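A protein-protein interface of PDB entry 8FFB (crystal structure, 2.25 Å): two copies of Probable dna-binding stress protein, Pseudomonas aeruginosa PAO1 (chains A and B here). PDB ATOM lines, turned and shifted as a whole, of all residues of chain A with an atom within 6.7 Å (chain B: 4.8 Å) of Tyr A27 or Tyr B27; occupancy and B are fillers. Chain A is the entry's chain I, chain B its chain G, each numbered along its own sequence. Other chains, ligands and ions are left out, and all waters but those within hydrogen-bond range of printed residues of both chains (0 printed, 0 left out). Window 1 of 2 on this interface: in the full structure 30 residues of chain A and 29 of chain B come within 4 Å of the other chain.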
ATOM      1  N   LEU A  22       8.030  19.264  26.023  1.00  0.00           N
ATOM      2  CA  LEU A  22       6.861  20.000  25.569  1.00  0.00           C
ATOM      3  C   LEU A  22       6.699  19.835  24.072  1.00  0.00           C
ATOM      4  O   LEU A  22       5.602  19.570  23.586  1.00  0.00           O
ATOM      5  CB  LEU A  22       6.974  21.478  25.934  1.00  0.00           C
ATOM      6  CG  LEU A  22       5.705  22.253  25.608  1.00  0.00           C
ATOM      7  CD1 LEU A  22       4.586  21.858  26.532  1.00  0.00           C
ATOM      8  CD2 LEU A  22       5.981  23.752  25.712  1.00  0.00           C
ATOM      9  N   LEU A  23       7.808  19.933  23.345  1.00  0.00           N
ATOM     10  CA  LEU A  23       7.819  19.719  21.906  1.00  0.00           C
ATOM     11  C   LEU A  23       7.253  18.356  21.533  1.00  0.00           C
ATOM     12  O   LEU A  23       6.322  18.252  20.722  1.00  0.00           O
ATOM     13  CB  LEU A  23       9.253  19.856  21.409  1.00  0.00           C
ATOM     14  CG  LEU A  23       9.463  19.688  19.920  1.00  0.00           C
ATOM     15  CD1 LEU A  23       8.563  20.659  19.165  1.00  0.00           C
ATOM     16  CD2 LEU A  23      10.888  19.974  19.604  1.00  0.00           C
ATOM     17  N   ALA A  24       7.806  17.289  22.118  1.00  0.00           N
ATOM     18  CA  ALA A  24       7.342  15.949  21.765  1.00  0.00           C
ATOM     19  C   ALA A  24       5.861  15.791  22.041  1.00  0.00           C
ATOM     20  O   ALA A  24       5.143  15.167  21.255  1.00  0.00           O
ATOM     21  CB  ALA A  24       8.130  14.888  22.531  1.00  0.00           C
ATOM     22  N   ASP A  25       5.386  16.326  23.172  1.00  0.00           N
ATOM     23  CA  ASP A  25       3.957  16.276  23.466  1.00  0.00           C
ATOM     24  C   ASP A  25       3.154  17.053  22.422  1.00  0.00           C
ATOM     25  O   ASP A  25       2.121  16.576  21.947  1.00  0.00           O
ATOM     26  CB  ASP A  25       3.685  16.826  24.861  1.00  0.00           C
ATOM     27  CG  ASP A  25       3.997  15.822  25.964  1.00  0.00           C
ATOM     28  OD1 ASP A  25       3.953  14.609  25.673  1.00  0.00           O
ATOM     29  OD2 ASP A  25       4.276  16.245  27.117  1.00  0.00           O
ATOM     30  N   THR A  26       3.613  18.254  22.055  1.00  0.00           N
ATOM     31  CA  THR A  26       2.883  19.043  21.069  1.00  0.00           C
ATOM     32  C   THR A  26       2.857  18.323  19.722  1.00  0.00           C
ATOM     33  O   THR A  26       1.810  18.234  19.076  1.00  0.00           O
ATOM     34  CB  THR A  26       3.507  20.443  20.954  1.00  0.00           C
ATOM     35  OG1 THR A  26       3.403  21.113  22.213  1.00  0.00           O
ATOM     36  CG2 THR A  26       2.793  21.286  19.934  1.00  0.00           C
ATOM     37  N   TYR A  27       3.989  17.787  19.286  1.00  0.00           N
ATOM     38  CA  TYR A  27       3.992  17.121  17.991  1.00  0.00           C
ATOM     39  C   TYR A  27       3.188  15.825  18.019  1.00  0.00           C
ATOM     40  O   TYR A  27       2.565  15.455  17.020  1.00  0.00           O
ATOM     41  CB  TYR A  27       5.424  16.850  17.548  1.00  0.00           C
ATOM     42  CG  TYR A  27       5.543  16.487  16.104  1.00  0.00           C
ATOM     43  CD1 TYR A  27       5.322  15.173  15.684  1.00  0.00           C
ATOM     44  CD2 TYR A  27       5.858  17.452  15.146  1.00  0.00           C
ATOM     45  CE1 TYR A  27       5.424  14.818  14.360  1.00  0.00           C
ATOM     46  CE2 TYR A  27       5.960  17.116  13.805  1.00  0.00           C
ATOM     47  CZ  TYR A  27       5.744  15.789  13.414  1.00  0.00           C
ATOM     48  OH  TYR A  27       5.849  15.414  12.082  1.00  0.00           O
ATOM     49  N   THR A  28       3.170  15.129  19.149  1.00  0.00           N
ATOM     50  CA  THR A  28       2.374  13.912  19.218  1.00  0.00           C
ATOM     51  C   THR A  28       0.896  14.237  19.114  1.00  0.00           C
ATOM     52  O   THR A  28       0.149  13.551  18.399  1.00  0.00           O
ATOM     53  CB  THR A  28       2.680  13.143  20.503  1.00  0.00           C
ATOM     54  OG1 THR A  28       4.050  12.740  20.488  1.00  0.00           O
ATOM     55  CG2 THR A  28       1.817  11.917  20.620  1.00  0.00           C
ATOM     56  N   LEU A  29       0.456  15.291  19.804  1.00  0.00           N
ATOM     57  CA  LEU A  29      -0.938  15.714  19.714  1.00  0.00           C
ATOM     58  C   LEU A  29      -1.250  16.202  18.314  1.00  0.00           C
ATOM     59  O   LEU A  29      -2.370  16.025  17.812  1.00  0.00           O
ATOM     60  CB  LEU A  29      -1.208  16.807  20.743  1.00  0.00           C
ATOM     61  CG  LEU A  29      -2.628  17.324  20.889  1.00  0.00           C
ATOM     62  CD1 LEU A  29      -3.523  16.176  21.230  1.00  0.00           C
ATOM     63  CD2 LEU A  29      -2.741  18.432  21.986  1.00  0.00           C
ATOM     64  N   TYR A  30      -0.258  16.813  17.674  1.00  0.00           N
ATOM     65  CA  TYR A  30      -0.363  17.171  16.271  1.00  0.00           C
ATOM     66  C   TYR A  30      -0.702  15.946  15.425  1.00  0.00           C
ATOM     67  O   TYR A  30      -1.745  15.902  14.766  1.00  0.00           O
ATOM     68  CB  TYR A  30       0.953  17.816  15.850  1.00  0.00           C
ATOM     69  CG  TYR A  30       1.125  18.080  14.389  1.00  0.00           C
ATOM     70  CD1 TYR A  30       0.378  19.053  13.742  1.00  0.00           C
ATOM     71  CD2 TYR A  30       2.056  17.385  13.659  1.00  0.00           C
ATOM     72  CE1 TYR A  30       0.539  19.301  12.402  1.00  0.00           C
ATOM     73  CE2 TYR A  30       2.232  17.629  12.316  1.00  0.00           C
ATOM     74  CZ  TYR A  30       1.468  18.591  11.690  1.00  0.00           C
ATOM     75  OH  TYR A  30       1.637  18.837  10.352  1.00  0.00           O
ATOM     76  N   LEU A  31       0.152  14.921  15.453  1.00  0.00           N
ATOM     77  CA  LEU A  31      -0.105  13.758  14.604  1.00  0.00           C
ATOM     78  C   LEU A  31      -1.443  13.117  14.956  1.00  0.00           C
ATOM     79  O   LEU A  31      -2.272  12.873  14.073  1.00  0.00           O
ATOM     80  CB  LEU A  31       1.043  12.761  14.698  1.00  0.00           C
ATOM     81  CG  LEU A  31       1.021  11.573  13.748  1.00  0.00           C
ATOM     82  CD1 LEU A  31       0.909  12.056  12.320  1.00  0.00           C
ATOM     83  CD2 LEU A  31       2.273  10.732  13.927  1.00  0.00           C
ATOM     84  N   LYS A  32      -1.715  12.899  16.243  1.00  0.00           N
ATOM     85  CA  LYS A  32      -3.000  12.307  16.604  1.00  0.00           C
ATOM     86  C   LYS A  32      -4.162  13.130  16.055  1.00  0.00           C
ATOM     87  O   LYS A  32      -5.129  12.574  15.520  1.00  0.00           O
ATOM     88  CB  LYS A  32      -3.135  12.155  18.123  1.00  0.00           C
ATOM     89  CG  LYS A  32      -4.512  11.633  18.547  1.00  0.00           C
ATOM     90  CD  LYS A  32      -4.661  11.410  20.048  1.00  0.00           C
ATOM     91  CE  LYS A  32      -3.805  10.264  20.546  1.00  0.00           C
ATOM     92  NZ  LYS A  32      -4.151  10.001  21.964  1.00  0.00           N
ATOM     93  N   HIS A  34      -4.214  15.149  13.493  1.00  0.00           N
ATOM     94  CA  HIS A  34      -4.201  14.939  12.049  1.00  0.00           C
ATOM     95  C   HIS A  34      -4.798  13.590  11.683  1.00  0.00           C
ATOM     96  O   HIS A  34      -5.542  13.471  10.704  1.00  0.00           O
ATOM     97  CB  HIS A  34      -2.762  15.025  11.549  1.00  0.00           C
ATOM     98  CG  HIS A  34      -2.629  15.646  10.209  1.00  0.00           C
ATOM     99  ND1 HIS A  34      -1.480  16.292   9.805  1.00  0.00           N
ATOM    100  CD2 HIS A  34      -3.509  15.751   9.187  1.00  0.00           C
ATOM    101  CE1 HIS A  34      -1.653  16.756   8.583  1.00  0.00           C
ATOM    102  NE2 HIS A  34      -2.873  16.435   8.182  1.00  0.00           N
ATOM    103  N   TRP A  38      -8.407  12.724   9.471  1.00  0.00           N
ATOM    104  CA  TRP A  38      -8.571  11.836   8.330  1.00  0.00           C
ATOM    105  C   TRP A  38      -9.674  10.808   8.570  1.00  0.00           C
ATOM    106  O   TRP A  38     -10.533  10.582   7.708  1.00  0.00           O
ATOM    107  CB  TRP A  38      -7.257  11.117   8.070  1.00  0.00           C
ATOM    108  CG  TRP A  38      -6.134  11.979   7.632  1.00  0.00           C
ATOM    109  CD1 TRP A  38      -6.218  13.106   6.877  1.00  0.00           C
ATOM    110  CD2 TRP A  38      -4.740  11.785   7.906  1.00  0.00           C
ATOM    111  NE1 TRP A  38      -4.966  13.623   6.655  1.00  0.00           N
ATOM    112  CE2 TRP A  38      -4.041  12.834   7.278  1.00  0.00           C
ATOM    113  CE3 TRP A  38      -4.018  10.827   8.616  1.00  0.00           C
ATOM    114  CZ2 TRP A  38      -2.661  12.951   7.336  1.00  0.00           C
ATOM    115  CZ3 TRP A  38      -2.646  10.947   8.668  1.00  0.00           C
ATOM    116  CH2 TRP A  38      -1.982  12.000   8.035  1.00  0.00           C
ATOM    117  N   LEU A  59      -1.220  23.698  15.809  1.00  0.00           N
ATOM    118  CA  LEU A  59      -0.155  22.934  16.464  1.00  0.00           C
ATOM    119  C   LEU A  59       1.129  22.915  15.636  1.00  0.00           C
ATOM    120  O   LEU A  59       2.232  22.932  16.206  1.00  0.00           O
ATOM    121  CB  LEU A  59      -0.624  21.494  16.758  1.00  0.00           C
ATOM    122  CG  LEU A  59      -1.762  21.378  17.760  1.00  0.00           C
ATOM    123  CD1 LEU A  59      -2.161  19.914  18.015  1.00  0.00           C
ATOM    124  CD2 LEU A  59      -1.357  22.053  19.053  1.00  0.00           C
ATOM    125  N   VAL A  63       4.758  23.718  17.202  1.00  0.00           N
ATOM    126  CA  VAL A  63       5.973  22.918  17.316  1.00  0.00           C
ATOM    127  C   VAL A  63       7.141  23.710  16.772  1.00  0.00           C
ATOM    128  O   VAL A  63       8.271  23.577  17.239  1.00  0.00           O
ATOM    129  CB  VAL A  63       5.858  21.549  16.606  1.00  0.00           C
ATOM    130  CG1 VAL A  63       4.523  20.893  16.876  1.00  0.00           C
ATOM    131  CG2 VAL A  63       6.092  21.671  15.143  1.00  0.00           C
ATOM    132  N   ILE A  66       8.242  26.204  19.612  1.00  0.00           N
ATOM    133  CA  ILE A  66       8.894  25.550  20.745  1.00  0.00           C
ATOM    134  C   ILE A  66      10.294  25.131  20.350  1.00  0.00           C
ATOM    135  O   ILE A  66      11.270  25.427  21.053  1.00  0.00           O
ATOM    136  CB  ILE A  66       8.065  24.356  21.237  1.00  0.00           C
ATOM    137  CG1 ILE A  66       6.698  24.862  21.707  1.00  0.00           C
ATOM    138  CG2 ILE A  66       8.860  23.576  22.340  1.00  0.00           C
ATOM    139  CD1 ILE A  66       5.542  23.812  21.609  1.00  0.00           C
ATOM    140  N   TYR A  81      10.909  10.294  15.224  1.00  0.00           N
ATOM    141  CA  TYR A  81       9.968   9.397  15.887  1.00  0.00           C
ATOM    142  C   TYR A  81      10.553   8.826  17.175  1.00  0.00           C
ATOM    143  O   TYR A  81       9.870   8.752  18.205  1.00  0.00           O
ATOM    144  CB  TYR A  81       9.592   8.242  14.956  1.00  0.00           C
ATOM    145  CG  TYR A  81       8.936   8.631  13.657  1.00  0.00           C
ATOM    146  CD1 TYR A  81       7.981   9.626  13.612  1.00  0.00           C
ATOM    147  CD2 TYR A  81       9.271   7.983  12.467  1.00  0.00           C
ATOM    148  CE1 TYR A  81       7.363   9.967  12.422  1.00  0.00           C
ATOM    149  CE2 TYR A  81       8.666   8.324  11.272  1.00  0.00           C
ATOM    150  CZ  TYR A  81       7.711   9.317  11.260  1.00  0.00           C
ATOM    151  OH  TYR A  81       7.105   9.670  10.085  1.00  0.00           O
ATOM    152  N   TYR A  84      10.703  11.484  19.937  1.00  0.00           N
ATOM    153  CA  TYR A  84       9.397  11.945  20.405  1.00  0.00           C
ATOM    154  C   TYR A  84       8.647  10.855  21.165  1.00  0.00           C
ATOM    155  O   TYR A  84       7.975  11.137  22.166  1.00  0.00           O
ATOM    156  CB  TYR A  84       8.572  12.454  19.226  1.00  0.00           C
ATOM    157  CG  TYR A  84       9.050  13.767  18.634  1.00  0.00           C
ATOM    158  CD1 TYR A  84       9.965  14.575  19.303  1.00  0.00           C
ATOM    159  CD2 TYR A  84       8.576  14.203  17.404  1.00  0.00           C
ATOM    160  CE1 TYR A  84      10.389  15.775  18.762  1.00  0.00           C
ATOM    161  CE2 TYR A  84       9.003  15.400  16.852  1.00  0.00           C
ATOM    162  CZ  TYR A  84       9.895  16.190  17.547  1.00  0.00           C
ATOM    163  OH  TYR A  84      10.318  17.382  17.016  1.00  0.00           O
ATOM    164  N   VAL A 113      -0.515  18.310  27.486  1.00  0.00           N
ATOM    165  CA  VAL A 113       0.457  19.369  27.188  1.00  0.00           C
ATOM    166  C   VAL A 113       0.478  20.422  28.298  1.00  0.00           C
ATOM    167  O   VAL A 113       1.541  20.889  28.707  1.00  0.00           O
ATOM    168  CB  VAL A 113       0.168  20.003  25.819  1.00  0.00           C
ATOM    169  CG1 VAL A 113       1.049  21.203  25.608  1.00  0.00           C
ATOM    170  CG2 VAL A 113       0.421  18.988  24.694  1.00  0.00           C
ATOM    171  N   LEU B  23       2.566   7.478   2.142  1.00  0.00           N
ATOM    172  CA  LEU B  23       2.248   8.383   3.244  1.00  0.00           C
ATOM    173  C   LEU B  23       3.338   8.358   4.307  1.00  0.00           C
ATOM    174  O   LEU B  23       3.787   9.411   4.774  1.00  0.00           O
ATOM    175  CB  LEU B  23       0.895   8.008   3.858  1.00  0.00           C
ATOM    176  CG  LEU B  23       0.482   8.841   5.067  1.00  0.00           C
ATOM    177  CD1 LEU B  23       0.504  10.308   4.734  1.00  0.00           C
ATOM    178  CD2 LEU B  23      -0.902   8.441   5.532  1.00  0.00           C
ATOM    179  N   ALA B  24       3.779   7.154   4.705  1.00  0.00           N
ATOM    180  CA  ALA B  24       4.750   7.041   5.788  1.00  0.00           C
ATOM    181  C   ALA B  24       6.107   7.595   5.375  1.00  0.00           C
ATOM    182  O   ALA B  24       6.835   8.152   6.208  1.00  0.00           O
ATOM    183  CB  ALA B  24       4.875   5.584   6.234  1.00  0.00           C
ATOM    184  N   ASP B  25       6.462   7.467   4.097  1.00  0.00           N
ATOM    185  CA  ASP B  25       7.727   8.023   3.645  1.00  0.00           C
ATOM    186  C   ASP B  25       7.642   9.528   3.608  1.00  0.00           C
ATOM    187  O   ASP B  25       8.538  10.219   4.093  1.00  0.00           O
ATOM    188  CB  ASP B  25       8.092   7.473   2.272  1.00  0.00           C
ATOM    189  CG  ASP B  25       8.447   6.011   2.327  1.00  0.00           C
ATOM    190  OD1 ASP B  25       8.994   5.587   3.371  1.00  0.00           O
ATOM    191  OD2 ASP B  25       8.153   5.285   1.360  1.00  0.00           O
ATOM    192  N   THR B  26       6.546  10.045   3.048  1.00  0.00           N
ATOM    193  CA  THR B  26       6.356  11.485   2.960  1.00  0.00           C
ATOM    194  C   THR B  26       6.347  12.118   4.350  1.00  0.00           C
ATOM    195  O   THR B  26       7.004  13.134   4.585  1.00  0.00           O
ATOM    196  CB  THR B  26       5.060  11.774   2.202  1.00  0.00           C
ATOM    197  OG1 THR B  26       5.123  11.161   0.911  1.00  0.00           O
ATOM    198  CG2 THR B  26       4.847  13.271   2.008  1.00  0.00           C
ATOM    199  N   TYR B  27       5.643  11.509   5.294  1.00  0.00           N
ATOM    200  CA  TYR B  27       5.575  12.098   6.618  1.00  0.00           C
ATOM    201  C   TYR B  27       6.917  12.035   7.316  1.00  0.00           C
ATOM    202  O   TYR B  27       7.276  12.951   8.057  1.00  0.00           O
ATOM    203  CB  TYR B  27       4.524  11.392   7.461  1.00  0.00           C
ATOM    204  CG  TYR B  27       4.018  12.286   8.544  1.00  0.00           C
ATOM    205  CD1 TYR B  27       4.651  12.328   9.789  1.00  0.00           C
ATOM    206  CD2 TYR B  27       2.932  13.128   8.313  1.00  0.00           C
ATOM    207  CE1 TYR B  27       4.190  13.162  10.782  1.00  0.00           C
ATOM    208  CE2 TYR B  27       2.464  13.965   9.284  1.00  0.00           C
ATOM    209  CZ  TYR B  27       3.093  13.981  10.516  1.00  0.00           C
ATOM    210  OH  TYR B  27       2.609  14.826  11.484  1.00  0.00           O
ATOM    211  N   THR B  28       7.645  10.937   7.130  1.00  0.00           N
ATOM    212  CA  THR B  28       8.961  10.800   7.742  1.00  0.00           C
ATOM    213  C   THR B  28       9.920  11.815   7.149  1.00  0.00           C
ATOM    214  O   THR B  28      10.726  12.425   7.868  1.00  0.00           O
ATOM    215  CB  THR B  28       9.479   9.372   7.527  1.00  0.00           C
ATOM    216  OG1 THR B  28       8.555   8.446   8.107  1.00  0.00           O
ATOM    217  CG2 THR B  28      10.837   9.165   8.135  1.00  0.00           C
ATOM    218  N   LEU B  29       9.829  12.016   5.835  1.00  0.00           N
ATOM    219  CA  LEU B  29      10.635  13.045   5.193  1.00  0.00           C
ATOM    220  C   LEU B  29      10.225  14.436   5.669  1.00  0.00           C
ATOM    221  O   LEU B  29      11.076  15.301   5.885  1.00  0.00           O
ATOM    222  CB  LEU B  29      10.499  12.926   3.683  1.00  0.00           C
ATOM    223  CG  LEU B  29      11.288  13.922   2.839  1.00  0.00           C
ATOM    224  CD1 LEU B  29      12.729  13.821   3.150  1.00  0.00           C
ATOM    225  CD2 LEU B  29      11.048  13.664   1.375  1.00  0.00           C
ATOM    226  N   TYR B  30       8.927  14.668   5.840  1.00  0.00           N
ATOM    227  CA  TYR B  30       8.462  15.942   6.374  1.00  0.00           C
ATOM    228  C   TYR B  30       9.128  16.249   7.709  1.00  0.00           C
ATOM    229  O   TYR B  30       9.736  17.314   7.883  1.00  0.00           O
ATOM    230  CB  TYR B  30       6.939  15.896   6.507  1.00  0.00           C
ATOM    231  CG  TYR B  30       6.321  16.929   7.430  1.00  0.00           C
ATOM    232  CD1 TYR B  30       5.934  18.157   6.944  1.00  0.00           C
ATOM    233  CD2 TYR B  30       6.088  16.656   8.774  1.00  0.00           C
ATOM    234  CE1 TYR B  30       5.343  19.097   7.753  1.00  0.00           C
ATOM    235  CE2 TYR B  30       5.501  17.606   9.608  1.00  0.00           C
ATOM    236  CZ  TYR B  30       5.121  18.821   9.077  1.00  0.00           C
ATOM    237  OH  TYR B  30       4.536  19.783   9.863  1.00  0.00           O
ATOM    238  N   LEU B  31       9.032  15.310   8.663  1.00  0.00           N
ATOM    239  CA  LEU B  31       9.624  15.515   9.979  1.00  0.00           C
ATOM    240  C   LEU B  31      11.113  15.760   9.879  1.00  0.00           C
ATOM    241  O   LEU B  31      11.653  16.645  10.555  1.00  0.00           O
ATOM    242  CB  LEU B  31       9.371  14.314  10.890  1.00  0.00           C
ATOM    243  CG  LEU B  31       9.900  14.497  12.310  1.00  0.00           C
ATOM    244  CD1 LEU B  31       9.323  15.782  12.905  1.00  0.00           C
ATOM    245  CD2 LEU B  31       9.572  13.289  13.193  1.00  0.00           C
ATOM    246  N   VAL B  63       1.075  15.031   2.574  1.00  0.00           N
ATOM    247  CA  VAL B  63       0.666  13.964   3.487  1.00  0.00           C
ATOM    248  C   VAL B  63      -0.843  13.972   3.605  1.00  0.00           C
ATOM    249  O   VAL B  63      -1.485  12.925   3.766  1.00  0.00           O
ATOM    250  CB  VAL B  63       1.336  14.088   4.879  1.00  0.00           C
ATOM    251  CG1 VAL B  63       2.856  13.892   4.798  1.00  0.00           C
ATOM    252  CG2 VAL B  63       1.009  15.429   5.540  1.00  0.00           C
ATOM    253  N   TYR B  81       3.547   7.237  15.188  1.00  0.00           N
ATOM    254  CA  TYR B  81       4.974   6.990  15.013  1.00  0.00           C
ATOM    255  C   TYR B  81       5.216   5.513  14.715  1.00  0.00           C
ATOM    256  O   TYR B  81       5.950   5.165  13.785  1.00  0.00           O
ATOM    257  CB  TYR B  81       5.755   7.412  16.255  1.00  0.00           C
ATOM    258  CG  TYR B  81       5.592   8.849  16.706  1.00  0.00           C
ATOM    259  CD1 TYR B  81       5.668   9.917  15.817  1.00  0.00           C
ATOM    260  CD2 TYR B  81       5.377   9.134  18.046  1.00  0.00           C
ATOM    261  CE1 TYR B  81       5.527  11.228  16.259  1.00  0.00           C
ATOM    262  CE2 TYR B  81       5.236  10.421  18.491  1.00  0.00           C
ATOM    263  CZ  TYR B  81       5.314  11.464  17.603  1.00  0.00           C
ATOM    264  OH  TYR B  81       5.161  12.731  18.107  1.00  0.00           O
ATOM    265  N   TYR B  84       4.258   4.548  11.188  1.00  0.00           N
ATOM    266  CA  TYR B  84       5.090   5.151  10.154  1.00  0.00           C
ATOM    267  C   TYR B  84       6.511   4.606  10.175  1.00  0.00           C
ATOM    268  O   TYR B  84       7.165   4.552   9.127  1.00  0.00           O
ATOM    269  CB  TYR B  84       5.118   6.671  10.299  1.00  0.00           C
ATOM    270  CG  TYR B  84       3.849   7.411   9.879  1.00  0.00           C
ATOM    271  CD1 TYR B  84       2.891   6.825   9.059  1.00  0.00           C
ATOM    272  CD2 TYR B  84       3.631   8.722  10.292  1.00  0.00           C
ATOM    273  CE1 TYR B  84       1.742   7.524   8.680  1.00  0.00           C
ATOM    274  CE2 TYR B  84       2.498   9.418   9.916  1.00  0.00           C
ATOM    275  CZ  TYR B  84       1.563   8.824   9.111  1.00  0.00           C
ATOM    276  OH  TYR B  84       0.439   9.536   8.767  1.00  0.00           O
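The backbone carbonyl oxygen (O) of Ala B24 lies within hydrogen-bond range of the side-chain hydroxyl (OG1) of Thr B28.
O of Ala A24 lies within hydrogen-bond range of OG1 of Thr A28 (2.8 Å).
O of Ala A24 touches OH of Tyr B81, 3.98 Å away.
Tyr A27 touches Leu B31.
CD1 of Tyr A27 touches OH of Tyr B81 (3.4 Å).
Tyr B81 touches Leu A31 (N to CD2, 3.9 Å).
CE2 of Tyr B84 touches CD1 of Leu A31 (3.9 Å).
Trp A38 touches Val B63.
Tyr A81 touches Tyr B27.
Leu B31 touches Tyr A81.
CD1 of Tyr A81 touches CD1 of Tyr B81, at 3.2 Å.
Tyr A81 touches Tyr B84 (OH to CB, 3.6 Å).
Of the 12 printed residues of chain B, 7 touch a printed residue of chain A.
Hydrophobic or aromatic side chains of chain B within 4 Å of the printed part of chain A: Tyr B27, Tyr B30, Leu B31, Tyr B81 and Tyr B84.
Of the 19 printed residues of chain A, 8 touch a printed residue of chain B.
Among the printed residues, 20 pairs touch across the chains.
OH of Tyr A27 sits close to OH of Tyr B27.
The side-chain hydroxyl (OH) of Tyr A81 lies within hydrogen-bond range of the side-chain hydroxyl (OG1) of Thr B28, 2.7 Å away.
OH of Tyr B30 sits at hydrogen-bond distance from OH of Tyr A30, 3.1 Å away.
OG1 of Thr A28 is in hydrogen-bond range of OH of Tyr B81 (2.6 Å).
Leu A22 touches none of the printed residues of chain B.
Asp A25 touches none of the printed residues of chain B.
Of the printed residues of chain B, Leu A31 touches Tyr B27 (3.4 Å), Tyr B81 (3.9 Å) and Tyr B84 (3.9 Å).
Of the printed residues of chain B, Tyr A81 touches Tyr B27 (3.6 Å), Thr B28 (2.7 Å), Leu B31 (3.9 Å), Tyr B81 (3.2 Å) and Tyr B84 (3.6 Å).
Of chain A, only Tyr A27, Tyr A30, Leu A31 and Tyr A81 come within 4 Å of Tyr B27.
Of the printed residues of chain A, Leu B31 touches Tyr A27 (3.6 Å), Tyr A81 (3.9 Å) and Tyr A84 (3.98 Å).
Of the printed residues of chain A, Val B63 touches Trp A38.
Of the printed residues of chain A, Tyr B84 touches Leu A31, Trp A38 and Tyr A81.
The nearest printed residue of chain B that does not touch Tyr A27 is Thr B28 (6.9 Å).
The nearest printed residue of chain A that does not touch Thr B28 is Tyr A27 (6.9 Å).
Tyr A27 touches Tyr B30, and with the chains exchanged Tyr A30 touches Tyr B27.
Tyr A27 touches Leu B31, and with the chains exchanged Leu A31 touches Tyr B27.
Leu A31 touches Tyr B81, and with the chains exchanged Tyr A81 touches Leu B31.
Tyr A81 touches Tyr B84, and with the chains exchanged Tyr A84 touches Tyr B81.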
